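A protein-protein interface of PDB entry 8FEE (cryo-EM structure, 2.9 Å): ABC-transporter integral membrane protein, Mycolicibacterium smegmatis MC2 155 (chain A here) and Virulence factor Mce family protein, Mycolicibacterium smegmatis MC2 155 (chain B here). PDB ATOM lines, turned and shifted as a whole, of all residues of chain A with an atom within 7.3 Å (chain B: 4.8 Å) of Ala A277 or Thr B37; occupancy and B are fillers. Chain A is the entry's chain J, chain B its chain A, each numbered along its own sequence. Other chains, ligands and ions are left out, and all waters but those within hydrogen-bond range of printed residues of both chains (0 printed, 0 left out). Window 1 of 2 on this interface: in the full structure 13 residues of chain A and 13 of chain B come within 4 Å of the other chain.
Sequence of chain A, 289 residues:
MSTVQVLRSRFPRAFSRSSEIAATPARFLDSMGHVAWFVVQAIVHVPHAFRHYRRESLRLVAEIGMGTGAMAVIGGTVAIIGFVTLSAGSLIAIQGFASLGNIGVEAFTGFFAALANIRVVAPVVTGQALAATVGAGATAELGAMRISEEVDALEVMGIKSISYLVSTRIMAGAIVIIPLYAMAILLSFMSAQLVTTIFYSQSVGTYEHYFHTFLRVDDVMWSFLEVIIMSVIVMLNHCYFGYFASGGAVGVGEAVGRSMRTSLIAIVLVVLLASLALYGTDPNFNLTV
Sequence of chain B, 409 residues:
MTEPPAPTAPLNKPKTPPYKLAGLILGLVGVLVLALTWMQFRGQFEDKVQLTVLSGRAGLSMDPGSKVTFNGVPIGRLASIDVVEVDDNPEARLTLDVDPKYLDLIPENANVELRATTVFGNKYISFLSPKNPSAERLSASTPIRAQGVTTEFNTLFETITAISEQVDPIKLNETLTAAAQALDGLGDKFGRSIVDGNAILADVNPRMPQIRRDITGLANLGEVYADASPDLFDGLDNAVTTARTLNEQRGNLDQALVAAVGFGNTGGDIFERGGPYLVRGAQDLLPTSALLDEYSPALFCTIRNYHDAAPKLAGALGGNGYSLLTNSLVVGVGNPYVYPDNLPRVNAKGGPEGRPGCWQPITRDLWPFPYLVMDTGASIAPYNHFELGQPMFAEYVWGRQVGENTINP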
ATOM      1  N   VAL A 271     -10.858  30.670  -2.390  1.00  0.00           N
ATOM      2  CA  VAL A 271     -10.104  30.952  -1.171  1.00  0.00           C
ATOM      3  C   VAL A 271     -11.010  30.860   0.050  1.00  0.00           C
ATOM      4  O   VAL A 271     -10.619  30.312   1.090  1.00  0.00           O
ATOM      5  CB  VAL A 271      -9.413  32.325  -1.265  1.00  0.00           C
ATOM      6  CG1 VAL A 271      -8.663  32.629   0.021  1.00  0.00           C
ATOM      7  CG2 VAL A 271      -8.460  32.351  -2.436  1.00  0.00           C
ATOM      8  N   LEU A 272     -12.240  31.376  -0.058  1.00  0.00           N
ATOM      9  CA  LEU A 272     -13.167  31.310   1.070  1.00  0.00           C
ATOM     10  C   LEU A 272     -13.464  29.867   1.460  1.00  0.00           C
ATOM     11  O   LEU A 272     -13.390  29.506   2.641  1.00  0.00           O
ATOM     12  CB  LEU A 272     -14.467  32.040   0.736  1.00  0.00           C
ATOM     13  CG  LEU A 272     -15.567  31.766   1.765  1.00  0.00           C
ATOM     14  CD1 LEU A 272     -15.200  32.379   3.106  1.00  0.00           C
ATOM     15  CD2 LEU A 272     -16.924  32.255   1.296  1.00  0.00           C
ATOM     16  N   LEU A 273     -13.806  29.027   0.477  1.00  0.00           N
ATOM     17  CA  LEU A 273     -14.150  27.641   0.779  1.00  0.00           C
ATOM     18  C   LEU A 273     -12.961  26.887   1.360  1.00  0.00           C
ATOM     19  O   LEU A 273     -13.112  26.119   2.319  1.00  0.00           O
ATOM     20  CB  LEU A 273     -14.665  26.937  -0.476  1.00  0.00           C
ATOM     21  CG  LEU A 273     -16.011  27.412  -1.024  1.00  0.00           C
ATOM     22  CD1 LEU A 273     -16.455  26.530  -2.178  1.00  0.00           C
ATOM     23  CD2 LEU A 273     -17.062  27.436   0.075  1.00  0.00           C
ATOM     24  N   ALA A 274     -11.771  27.093   0.793  1.00  0.00           N
ATOM     25  CA  ALA A 274     -10.593  26.393   1.290  1.00  0.00           C
ATOM     26  C   ALA A 274     -10.259  26.804   2.718  1.00  0.00           C
ATOM     27  O   ALA A 274      -9.922  25.954   3.553  1.00  0.00           O
ATOM     28  CB  ALA A 274      -9.411  26.645   0.362  1.00  0.00           C
ATOM     29  N   SER A 275     -10.344  28.102   3.025  1.00  0.00           N
ATOM     30  CA  SER A 275     -10.063  28.550   4.386  1.00  0.00           C
ATOM     31  C   SER A 275     -11.121  28.059   5.366  1.00  0.00           C
ATOM     32  O   SER A 275     -10.805  27.746   6.519  1.00  0.00           O
ATOM     33  CB  SER A 275      -9.953  30.072   4.429  1.00  0.00           C
ATOM     34  OG  SER A 275      -8.663  30.500   4.032  1.00  0.00           O
ATOM     35  N   LEU A 276     -12.384  27.998   4.933  1.00  0.00           N
ATOM     36  CA  LEU A 276     -13.433  27.471   5.802  1.00  0.00           C
ATOM     37  C   LEU A 276     -13.217  25.993   6.097  1.00  0.00           C
ATOM     38  O   LEU A 276     -13.453  25.539   7.222  1.00  0.00           O
ATOM     39  CB  LEU A 276     -14.804  27.696   5.166  1.00  0.00           C
ATOM     40  CG  LEU A 276     -15.718  28.680   5.894  1.00  0.00           C
ATOM     41  CD1 LEU A 276     -15.033  30.024   6.046  1.00  0.00           C
ATOM     42  CD2 LEU A 276     -17.040  28.827   5.161  1.00  0.00           C
ATOM     43  N   ALA A 277     -12.777  25.227   5.097  1.00  0.00           N
ATOM     44  CA  ALA A 277     -12.558  23.799   5.308  1.00  0.00           C
ATOM     45  C   ALA A 277     -11.329  23.541   6.172  1.00  0.00           C
ATOM     46  O   ALA A 277     -11.373  22.707   7.085  1.00  0.00           O
ATOM     47  CB  ALA A 277     -12.428  23.084   3.965  1.00  0.00           C
ATOM     48  N   LEU A 278     -10.225  24.242   5.904  1.00  0.00           N
ATOM     49  CA  LEU A 278      -8.972  23.957   6.598  1.00  0.00           C
ATOM     50  C   LEU A 278      -9.044  24.315   8.079  1.00  0.00           C
ATOM     51  O   LEU A 278      -8.654  23.517   8.939  1.00  0.00           O
ATOM     52  CB  LEU A 278      -7.826  24.706   5.923  1.00  0.00           C
ATOM     53  CG  LEU A 278      -7.355  24.135   4.589  1.00  0.00           C
ATOM     54  CD1 LEU A 278      -6.514  25.158   3.861  1.00  0.00           C
ATOM     55  CD2 LEU A 278      -6.569  22.856   4.812  1.00  0.00           C
ATOM     56  N   TYR A 279      -9.534  25.512   8.400  1.00  0.00           N
ATOM     57  CA  TYR A 279      -9.494  26.037   9.759  1.00  0.00           C
ATOM     58  C   TYR A 279     -10.881  26.132  10.386  1.00  0.00           C
ATOM     59  O   TYR A 279     -11.115  26.970  11.259  1.00  0.00           O
ATOM     60  CB  TYR A 279      -8.810  27.403   9.780  1.00  0.00           C
ATOM     61  CG  TYR A 279      -7.546  27.456   8.959  1.00  0.00           C
ATOM     62  CD1 TYR A 279      -6.375  26.874   9.417  1.00  0.00           C
ATOM     63  CD2 TYR A 279      -7.524  28.086   7.724  1.00  0.00           C
ATOM     64  CE1 TYR A 279      -5.219  26.916   8.669  1.00  0.00           C
ATOM     65  CE2 TYR A 279      -6.371  28.135   6.969  1.00  0.00           C
ATOM     66  CZ  TYR A 279      -5.222  27.548   7.447  1.00  0.00           C
ATOM     67  OH  TYR A 279      -4.068  27.593   6.699  1.00  0.00           O
ATOM     68  N   GLY A 280     -11.810  25.284   9.944  1.00  0.00           N
ATOM     69  CA  GLY A 280     -13.159  25.337  10.482  1.00  0.00           C
ATOM     70  C   GLY A 280     -13.231  24.982  11.955  1.00  0.00           C
ATOM     71  O   GLY A 280     -13.909  25.659  12.733  1.00  0.00           O
ATOM     72  N   THR A 281     -12.536  23.923  12.359  1.00  0.00           N
ATOM     73  CA  THR A 281     -12.542  23.467  13.744  1.00  0.00           C
ATOM     74  C   THR A 281     -11.243  23.758  14.475  1.00  0.00           C
ATOM     75  O   THR A 281     -11.275  24.213  15.621  1.00  0.00           O
ATOM     76  CB  THR A 281     -12.828  21.961  13.802  1.00  0.00           C
ATOM     77  OG1 THR A 281     -14.058  21.683  13.118  1.00  0.00           O
ATOM     78  CG2 THR A 281     -12.947  21.491  15.244  1.00  0.00           C
ATOM     79  N   ASP A 282     -10.099  23.525  13.838  1.00  0.00           N
ATOM     80  CA  ASP A 282      -8.806  23.796  14.454  1.00  0.00           C
ATOM     81  C   ASP A 282      -8.210  25.048  13.829  1.00  0.00           C
ATOM     82  O   ASP A 282      -7.784  25.010  12.664  1.00  0.00           O
ATOM     83  CB  ASP A 282      -7.861  22.606  14.275  1.00  0.00           C
ATOM     84  CG  ASP A 282      -6.563  22.773  15.039  1.00  0.00           C
ATOM     85  OD1 ASP A 282      -6.517  23.615  15.961  1.00  0.00           O
ATOM     86  OD2 ASP A 282      -5.589  22.062  14.717  1.00  0.00           O
ATOM     87  N   VAL B  33     -19.308  19.445  -3.292  1.00  0.00           N
ATOM     88  CA  VAL B  33     -18.157  20.150  -2.731  1.00  0.00           C
ATOM     89  C   VAL B  33     -18.604  21.126  -1.650  1.00  0.00           C
ATOM     90  O   VAL B  33     -17.983  21.221  -0.582  1.00  0.00           O
ATOM     91  CB  VAL B  33     -17.364  20.855  -3.849  1.00  0.00           C
ATOM     92  CG1 VAL B  33     -16.439  21.916  -3.273  1.00  0.00           C
ATOM     93  CG2 VAL B  33     -16.561  19.837  -4.645  1.00  0.00           C
ATOM     94  N   LEU B  34     -19.692  21.862  -1.904  1.00  0.00           N
ATOM     95  CA  LEU B  34     -20.219  22.778  -0.894  1.00  0.00           C
ATOM     96  C   LEU B  34     -20.638  22.032   0.369  1.00  0.00           C
ATOM     97  O   LEU B  34     -20.330  22.463   1.488  1.00  0.00           O
ATOM     98  CB  LEU B  34     -21.393  23.575  -1.462  1.00  0.00           C
ATOM     99  CG  LEU B  34     -21.093  24.980  -1.993  1.00  0.00           C
ATOM    100  CD1 LEU B  34     -20.120  24.941  -3.163  1.00  0.00           C
ATOM    101  CD2 LEU B  34     -22.381  25.689  -2.384  1.00  0.00           C
ATOM    102  N   ALA B  35     -21.340  20.907   0.211  1.00  0.00           N
ATOM    103  CA  ALA B  35     -21.770  20.137   1.374  1.00  0.00           C
ATOM    104  C   ALA B  35     -20.578  19.581   2.142  1.00  0.00           C
ATOM    105  O   ALA B  35     -20.565  19.598   3.378  1.00  0.00           O
ATOM    106  CB  ALA B  35     -22.704  19.007   0.940  1.00  0.00           C
ATOM    107  N   LEU B  36     -19.566  19.083   1.426  1.00  0.00           N
ATOM    108  CA  LEU B  36     -18.390  18.518   2.081  1.00  0.00           C
ATOM    109  C   LEU B  36     -17.608  19.577   2.848  1.00  0.00           C
ATOM    110  O   LEU B  36     -17.168  19.327   3.975  1.00  0.00           O
ATOM    111  CB  LEU B  36     -17.494  17.826   1.054  1.00  0.00           C
ATOM    112  CG  LEU B  36     -17.640  16.309   0.899  1.00  0.00           C
ATOM    113  CD1 LEU B  36     -19.074  15.900   0.595  1.00  0.00           C
ATOM    114  CD2 LEU B  36     -16.697  15.794  -0.179  1.00  0.00           C
ATOM    115  N   THR B  37     -17.416  20.763   2.260  1.00  0.00           N
ATOM    116  CA  THR B  37     -16.707  21.807   2.995  1.00  0.00           C
ATOM    117  C   THR B  37     -17.530  22.333   4.168  1.00  0.00           C
ATOM    118  O   THR B  37     -16.958  22.677   5.207  1.00  0.00           O
ATOM    119  CB  THR B  37     -16.272  22.953   2.072  1.00  0.00           C
ATOM    120  OG1 THR B  37     -15.526  23.914   2.830  1.00  0.00           O
ATOM    121  CG2 THR B  37     -17.453  23.654   1.442  1.00  0.00           C
ATOM    122  N   TRP B  38     -18.863  22.370   4.047  1.00  0.00           N
ATOM    123  CA  TRP B  38     -19.686  22.739   5.196  1.00  0.00           C
ATOM    124  C   TRP B  38     -19.575  21.715   6.321  1.00  0.00           C
ATOM    125  O   TRP B  38     -19.477  22.084   7.498  1.00  0.00           O
ATOM    126  CB  TRP B  38     -21.143  22.907   4.768  1.00  0.00           C
ATOM    127  CG  TRP B  38     -22.039  23.350   5.882  1.00  0.00           C
ATOM    128  CD1 TRP B  38     -22.982  22.601   6.523  1.00  0.00           C
ATOM    129  CD2 TRP B  38     -22.067  24.645   6.498  1.00  0.00           C
ATOM    130  NE1 TRP B  38     -23.601  23.351   7.494  1.00  0.00           N
ATOM    131  CE2 TRP B  38     -23.057  24.608   7.500  1.00  0.00           C
ATOM    132  CE3 TRP B  38     -21.354  25.830   6.296  1.00  0.00           C
ATOM    133  CZ2 TRP B  38     -23.351  25.711   8.299  1.00  0.00           C
ATOM    134  CZ3 TRP B  38     -21.647  26.924   7.090  1.00  0.00           C
ATOM    135  CH2 TRP B  38     -22.637  26.857   8.079  1.00  0.00           C
ATOM    136  N   MET B  39     -19.589  20.423   5.981  1.00  0.00           N
ATOM    137  CA  MET B  39     -19.446  19.386   7.001  1.00  0.00           C
ATOM    138  C   MET B  39     -18.066  19.425   7.647  1.00  0.00           C
ATOM    139  O   MET B  39     -17.939  19.229   8.861  1.00  0.00           O
ATOM    140  CB  MET B  39     -19.721  18.008   6.398  1.00  0.00           C
ATOM    141  CG  MET B  39     -21.163  17.796   5.968  1.00  0.00           C
ATOM    142  SD  MET B  39     -21.437  16.182   5.216  1.00  0.00           S
ATOM    143  CE  MET B  39     -20.958  15.098   6.557  1.00  0.00           C
ATOM    144  N   GLN B  40     -17.022  19.661   6.849  1.00  0.00           N
ATOM    145  CA  GLN B  40     -15.677  19.781   7.404  1.00  0.00           C
ATOM    146  C   GLN B  40     -15.566  20.998   8.315  1.00  0.00           C
ATOM    147  O   GLN B  40     -14.900  20.944   9.357  1.00  0.00           O
ATOM    148  CB  GLN B  40     -14.651  19.850   6.272  1.00  0.00           C
ATOM    149  CG  GLN B  40     -13.217  20.090   6.722  1.00  0.00           C
ATOM    150  CD  GLN B  40     -12.593  18.889   7.411  1.00  0.00           C
ATOM    151  OE1 GLN B  40     -13.165  17.800   7.433  1.00  0.00           O
ATOM    152  NE2 GLN B  40     -11.408  19.087   7.976  1.00  0.00           N
ATOM    153  N   PHE B  41     -16.204  22.108   7.935  1.00  0.00           N
ATOM    154  CA  PHE B  41     -16.225  23.289   8.791  1.00  0.00           C
ATOM    155  C   PHE B  41     -16.944  23.002  10.104  1.00  0.00           C
ATOM    156  O   PHE B  41     -16.498  23.432  11.173  1.00  0.00           O
ATOM    157  CB  PHE B  41     -16.889  24.451   8.052  1.00  0.00           C
ATOM    158  CG  PHE B  41     -17.191  25.634   8.923  1.00  0.00           C
ATOM    159  CD1 PHE B  41     -16.180  26.487   9.323  1.00  0.00           C
ATOM    160  CD2 PHE B  41     -18.486  25.896   9.336  1.00  0.00           C
ATOM    161  CE1 PHE B  41     -16.448  27.575  10.125  1.00  0.00           C
ATOM    162  CE2 PHE B  41     -18.761  26.985  10.138  1.00  0.00           C
ATOM    163  CZ  PHE B  41     -17.739  27.824  10.532  1.00  0.00           C
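Leu A276 touches Phe B41 (O to CD1, 3.6 Å). Thr B37 touches Ala A277. Ala A277 touches Gln B40. CD1 of Phe B41 touches CA of Gly A280, 3.4 Å away. Thr A281 touches Gln B40. O of Phe B41 touches OG1 of Thr A281, at 3.6 Å.
Of the printed residues of chain B, Leu A273 touches Thr B37 (3.3 Å). Of the printed residues of chain B, Leu A276 touches Phe B41. Printed residues of chain B within 4 Å of Ala A277: Thr B37 (3.4 Å) and Gln B40 (3.2 Å). Of the printed residues of chain B, Gly A280 touches Phe B41 (3.4 Å). Printed residues of chain B within 4 Å of Thr A281: Gln B40 and Phe B41. Thr B37 touches just these residues of chain A: Leu A273 and Ala A277. Of the printed residues of chain A, Phe B41 touches Leu A276, Gly A280 and Thr A281. The nearest printed residue of chain B that does not touch Ala A277 is Phe B41 (4.8 Å).
Of the 9 printed residues of chain B, 3 touch a printed residue of chain A. Hydrophobic or aromatic side chains of chain B within 4 Å of the printed part of chain A: Phe B41. Of the 12 printed residues of chain A, 5 touch a printed residue of chain B. Hydrophobic or aromatic side chains of chain A within 4 Å of the printed part of chain B: Ala A277. Along chain A the printed residues that touch a printed residue of chain B span positions 273 to 281. Among the printed residues, no Asp or Glu carboxylate lies within 4 Å of a Lys or Arg side-chain nitrogen of the other chain.
OG1 of Thr B37 is in hydrogen-bond range of O of Leu A273 (3.3 Å).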
